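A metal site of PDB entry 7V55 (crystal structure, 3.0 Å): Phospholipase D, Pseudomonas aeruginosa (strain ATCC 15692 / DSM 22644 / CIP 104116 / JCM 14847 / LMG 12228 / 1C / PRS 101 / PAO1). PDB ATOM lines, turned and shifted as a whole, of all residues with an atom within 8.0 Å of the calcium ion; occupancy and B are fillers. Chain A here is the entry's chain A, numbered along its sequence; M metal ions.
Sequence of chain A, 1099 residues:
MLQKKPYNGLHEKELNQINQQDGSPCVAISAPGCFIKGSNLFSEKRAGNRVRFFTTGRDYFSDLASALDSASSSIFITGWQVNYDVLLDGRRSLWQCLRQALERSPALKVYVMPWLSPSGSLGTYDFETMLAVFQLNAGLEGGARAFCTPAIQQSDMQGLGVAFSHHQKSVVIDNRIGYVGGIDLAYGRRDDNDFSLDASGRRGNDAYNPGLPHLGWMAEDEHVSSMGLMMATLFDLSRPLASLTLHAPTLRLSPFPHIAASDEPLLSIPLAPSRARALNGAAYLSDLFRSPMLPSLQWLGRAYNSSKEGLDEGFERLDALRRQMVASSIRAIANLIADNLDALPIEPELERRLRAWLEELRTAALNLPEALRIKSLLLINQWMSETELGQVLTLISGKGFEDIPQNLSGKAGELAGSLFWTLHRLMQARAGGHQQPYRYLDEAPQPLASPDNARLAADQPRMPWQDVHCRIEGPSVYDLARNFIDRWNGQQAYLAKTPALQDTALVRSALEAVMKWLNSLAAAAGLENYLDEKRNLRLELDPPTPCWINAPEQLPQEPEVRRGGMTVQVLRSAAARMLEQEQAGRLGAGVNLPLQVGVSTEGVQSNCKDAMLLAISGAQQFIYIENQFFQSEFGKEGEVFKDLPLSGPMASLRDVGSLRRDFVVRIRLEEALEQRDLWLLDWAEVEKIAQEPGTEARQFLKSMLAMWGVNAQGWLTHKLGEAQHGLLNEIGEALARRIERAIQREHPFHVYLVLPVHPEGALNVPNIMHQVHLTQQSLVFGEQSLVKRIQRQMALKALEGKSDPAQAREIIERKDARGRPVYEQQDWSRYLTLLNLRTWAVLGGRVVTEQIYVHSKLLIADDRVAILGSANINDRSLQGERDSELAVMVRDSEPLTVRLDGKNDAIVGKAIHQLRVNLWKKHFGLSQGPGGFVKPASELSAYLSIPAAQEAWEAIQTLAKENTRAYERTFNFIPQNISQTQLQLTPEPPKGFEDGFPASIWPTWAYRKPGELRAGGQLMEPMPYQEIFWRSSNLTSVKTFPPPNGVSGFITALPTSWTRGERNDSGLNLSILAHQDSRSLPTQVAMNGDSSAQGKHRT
The side-chain carboxylate (OD2) of Asp 194 lies close to the backbone NH (N) of Gly 929 (3.4 Å). OE1 of Gln 928 lies close to O of Val 934 (2.7 Å). The side-chain carboxylate (OD1) of Asp 192 lies within hydrogen-bond range of the backbone NH (N) of Asp 194 (3.1 Å).
Residues that only touch the calcium ion: Gly 932 (3.96 Å).
The calcium ion is bound by NE2 of Gln 928, at 2.3 Å. The calcium ion is bound by OD2 of Asp 194, 2.4 Å away. The backbone carbonyl oxygen (O) of Gly 931 binds the calcium ion, 2.6 Å away. The calcium ion has three donor atoms within binding distance. Slightly farther from the calcium ion lies the backbone carbonyl oxygen (O) of Gly 929 (2.9 Å).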
ATOM      1  N   ASP A 192      28.768  22.724  -0.666  1.00  0.00           N
ATOM      2  CA  ASP A 192      29.257  23.097   0.656  1.00  0.00           C
ATOM      3  C   ASP A 192      28.941  21.963   1.615  1.00  0.00           C
ATOM      4  O   ASP A 192      28.616  20.846   1.204  1.00  0.00           O
ATOM      5  CB  ASP A 192      28.640  24.399   1.181  1.00  0.00           C
ATOM      6  CG  ASP A 192      27.147  24.557   0.861  1.00  0.00           C
ATOM      7  OD1 ASP A 192      26.385  23.551   0.886  1.00  0.00           O
ATOM      8  OD2 ASP A 192      26.736  25.722   0.682  1.00  0.00           O
ATOM      9  N   ASN A 193      29.006  22.283   2.914  1.00  0.00           N
ATOM     10  CA  ASN A 193      28.637  21.351   3.980  1.00  0.00           C
ATOM     11  C   ASN A 193      27.146  21.359   4.297  1.00  0.00           C
ATOM     12  O   ASN A 193      26.718  20.558   5.131  1.00  0.00           O
ATOM     13  CB  ASN A 193      29.425  21.622   5.265  1.00  0.00           C
ATOM     14  CG  ASN A 193      30.901  21.809   5.013  1.00  0.00           C
ATOM     15  OD1 ASN A 193      31.639  20.827   4.963  1.00  0.00           O
ATOM     16  ND2 ASN A 193      31.344  23.047   4.917  1.00  0.00           N
ATOM     17  N   ASP A 194      26.342  22.219   3.685  1.00  0.00           N
ATOM     18  CA  ASP A 194      24.933  22.058   3.961  1.00  0.00           C
ATOM     19  C   ASP A 194      24.339  20.894   3.208  1.00  0.00           C
ATOM     20  O   ASP A 194      23.345  20.324   3.668  1.00  0.00           O
ATOM     21  CB  ASP A 194      24.123  23.329   3.671  1.00  0.00           C
ATOM     22  CG  ASP A 194      24.561  24.524   4.485  1.00  0.00           C
ATOM     23  OD1 ASP A 194      25.715  24.979   4.428  1.00  0.00           O
ATOM     24  OD2 ASP A 194      23.702  25.002   5.239  1.00  0.00           O
ATOM     25  N   PHE A 195      24.910  20.508   2.066  1.00  0.00           N
ATOM     26  CA  PHE A 195      24.349  19.420   1.268  1.00  0.00           C
ATOM     27  C   PHE A 195      22.897  19.724   0.918  1.00  0.00           C
ATOM     28  O   PHE A 195      22.010  18.885   1.048  1.00  0.00           O
ATOM     29  CB  PHE A 195      24.474  18.076   2.001  1.00  0.00           C
ATOM     30  CG  PHE A 195      25.848  17.462   1.969  1.00  0.00           C
ATOM     31  CD1 PHE A 195      26.623  17.492   0.835  1.00  0.00           C
ATOM     32  CD2 PHE A 195      26.383  16.869   3.106  1.00  0.00           C
ATOM     33  CE1 PHE A 195      27.888  16.930   0.830  1.00  0.00           C
ATOM     34  CE2 PHE A 195      27.643  16.329   3.106  1.00  0.00           C
ATOM     35  CZ  PHE A 195      28.392  16.345   1.967  1.00  0.00           C
ATOM     36  N   SER A 196      22.647  20.963   0.497  1.00  0.00           N
ATOM     37  CA  SER A 196      21.269  21.371   0.280  1.00  0.00           C
ATOM     38  C   SER A 196      20.671  20.629  -0.917  1.00  0.00           C
ATOM     39  O   SER A 196      21.384  20.154  -1.794  1.00  0.00           O
ATOM     40  CB  SER A 196      21.188  22.867   0.020  1.00  0.00           C
ATOM     41  OG  SER A 196      19.837  23.207  -0.169  1.00  0.00           O
ATOM     42  N   GLY A 925      26.977  16.507  10.173  1.00  0.00           N
ATOM     43  CA  GLY A 925      26.126  17.664  10.294  1.00  0.00           C
ATOM     44  C   GLY A 925      26.652  18.746  11.186  1.00  0.00           C
ATOM     45  O   GLY A 925      25.974  19.763  11.368  1.00  0.00           O
ATOM     46  N   SER A 927      28.990  20.784  10.661  1.00  0.00           N
ATOM     47  CA  SER A 927      29.676  21.785   9.871  1.00  0.00           C
ATOM     48  C   SER A 927      28.730  22.628   9.060  1.00  0.00           C
ATOM     49  O   SER A 927      29.140  23.671   8.515  1.00  0.00           O
ATOM     50  CB  SER A 927      30.681  21.108   8.929  1.00  0.00           C
ATOM     51  OG  SER A 927      31.954  21.060   9.525  1.00  0.00           O
ATOM     52  N   GLN A 928      27.463  22.222   8.967  1.00  0.00           N
ATOM     53  CA  GLN A 928      26.520  23.004   8.170  1.00  0.00           C
ATOM     54  C   GLN A 928      26.298  24.352   8.830  1.00  0.00           C
ATOM     55  O   GLN A 928      26.839  24.660   9.889  1.00  0.00           O
ATOM     56  CB  GLN A 928      25.202  22.254   7.967  1.00  0.00           C
ATOM     57  CG  GLN A 928      24.181  22.358   9.051  1.00  0.00           C
ATOM     58  CD  GLN A 928      23.062  21.371   8.851  1.00  0.00           C
ATOM     59  OE1 GLN A 928      22.973  20.360   9.542  1.00  0.00           O
ATOM     60  NE2 GLN A 928      22.197  21.671   7.871  1.00  0.00           N
ATOM     61  N   GLY A 929      25.517  25.178   8.145  1.00  0.00           N
ATOM     62  CA  GLY A 929      25.161  26.476   8.653  1.00  0.00           C
ATOM     63  C   GLY A 929      23.655  26.606   8.744  1.00  0.00           C
ATOM     64  O   GLY A 929      22.907  25.610   8.671  1.00  0.00           O
ATOM     65  N   PRO A 930      23.178  27.837   8.884  1.00  0.00           N
ATOM     66  CA  PRO A 930      21.728  28.066   9.019  1.00  0.00           C
ATOM     67  C   PRO A 930      20.988  27.425   7.854  1.00  0.00           C
ATOM     68  O   PRO A 930      21.399  27.532   6.701  1.00  0.00           O
ATOM     69  CB  PRO A 930      21.608  29.585   8.993  1.00  0.00           C
ATOM     70  CG  PRO A 930      22.948  30.088   9.450  1.00  0.00           C
ATOM     71  CD  PRO A 930      23.929  29.100   8.865  1.00  0.00           C
ATOM     72  N   GLY A 931      19.920  26.721   8.167  1.00  0.00           N
ATOM     73  CA  GLY A 931      19.054  26.163   7.152  1.00  0.00           C
ATOM     74  C   GLY A 931      19.232  24.667   7.047  1.00  0.00           C
ATOM     75  O   GLY A 931      20.047  24.048   7.741  1.00  0.00           O
ATOM     76  N   GLY A 932      18.468  24.095   6.126  1.00  0.00           N
ATOM     77  CA  GLY A 932      18.448  22.664   5.898  1.00  0.00           C
ATOM     78  C   GLY A 932      17.400  21.992   6.753  1.00  0.00           C
ATOM     79  O   GLY A 932      16.787  22.589   7.633  1.00  0.00           O
ATOM     80  N   PHE A 933      17.192  20.704   6.480  1.00  0.00           N
ATOM     81  CA  PHE A 933      16.218  19.948   7.253  1.00  0.00           C
ATOM     82  C   PHE A 933      16.831  18.857   8.112  1.00  0.00           C
ATOM     83  O   PHE A 933      16.104  17.994   8.622  1.00  0.00           O
ATOM     84  CB  PHE A 933      15.174  19.334   6.319  1.00  0.00           C
ATOM     85  CG  PHE A 933      14.247  20.351   5.758  1.00  0.00           C
ATOM     86  CD1 PHE A 933      13.161  20.794   6.494  1.00  0.00           C
ATOM     87  CD2 PHE A 933      14.460  20.881   4.493  1.00  0.00           C
ATOM     88  CE1 PHE A 933      12.314  21.752   5.988  1.00  0.00           C
ATOM     89  CE2 PHE A 933      13.606  21.831   3.967  1.00  0.00           C
ATOM     90  CZ  PHE A 933      12.526  22.273   4.722  1.00  0.00           C
ATOM     91  N   VAL A 934      18.151  18.881   8.312  1.00  0.00           N
ATOM     92  CA  VAL A 934      18.833  17.799   9.014  1.00  0.00           C
ATOM     93  C   VAL A 934      19.637  18.366  10.164  1.00  0.00           C
ATOM     94  O   VAL A 934      20.596  19.111   9.951  1.00  0.00           O
ATOM     95  CB  VAL A 934      19.737  17.000   8.070  1.00  0.00           C
ATOM     96  CG1 VAL A 934      20.556  16.029   8.899  1.00  0.00           C
ATOM     97  CG2 VAL A 934      18.888  16.265   7.055  1.00  0.00           C
ATOM     98  N   LYS A 935      19.258  17.984  11.388  1.00  0.00           N
ATOM     99  CA  LYS A 935      19.854  18.574  12.571  1.00  0.00           C
ATOM    100  C   LYS A 935      21.303  18.101  12.750  1.00  0.00           C
ATOM    101  O   LYS A 935      21.638  16.967  12.410  1.00  0.00           O
ATOM    102  CB  LYS A 935      19.029  18.224  13.818  1.00  0.00           C
ATOM    103  CG  LYS A 935      18.846  16.724  13.990  1.00  0.00           C
ATOM    104  CD  LYS A 935      17.740  16.338  14.983  1.00  0.00           C
ATOM    105  CE  LYS A 935      17.828  17.061  16.301  1.00  0.00           C
ATOM    106  NZ  LYS A 935      16.538  16.935  17.027  1.00  0.00           N
ATOM    107  N   PRO A 936      22.168  18.969  13.269  1.00  0.00           N
ATOM    108  CA  PRO A 936      23.500  18.525  13.664  1.00  0.00           C
ATOM    109  C   PRO A 936      23.429  17.340  14.617  1.00  0.00           C
ATOM    110  O   PRO A 936      22.630  17.339  15.562  1.00  0.00           O
ATOM    111  CB  PRO A 936      24.071  19.757  14.367  1.00  0.00           C
ATOM    112  CG  PRO A 936      23.388  20.910  13.682  1.00  0.00           C
ATOM    113  CD  PRO A 936      21.984  20.413  13.486  1.00  0.00           C
ATOM    114  N   PHE A1050      24.085  13.145   8.376  1.00  0.00           N
ATOM    115  CA  PHE A1050      23.871  12.633   7.032  1.00  0.00           C
ATOM    116  C   PHE A1050      24.206  11.176   6.893  1.00  0.00           C
ATOM    117  O   PHE A1050      24.061  10.612   5.796  1.00  0.00           O
ATOM    118  CB  PHE A1050      24.675  13.441   6.032  1.00  0.00           C
ATOM    119  CG  PHE A1050      24.398  14.866   6.108  1.00  0.00           C
ATOM    120  CD1 PHE A1050      23.147  15.343   5.775  1.00  0.00           C
ATOM    121  CD2 PHE A1050      25.359  15.748   6.515  1.00  0.00           C
ATOM    122  CE1 PHE A1050      22.868  16.677   5.833  1.00  0.00           C
ATOM    123  CE2 PHE A1050      25.091  17.090   6.570  1.00  0.00           C
ATOM    124  CZ  PHE A1050      23.838  17.557   6.237  1.00  0.00           C
HETATM  125 CA    CA M   1      22.353  23.571   6.663  1.00  0.00          CA
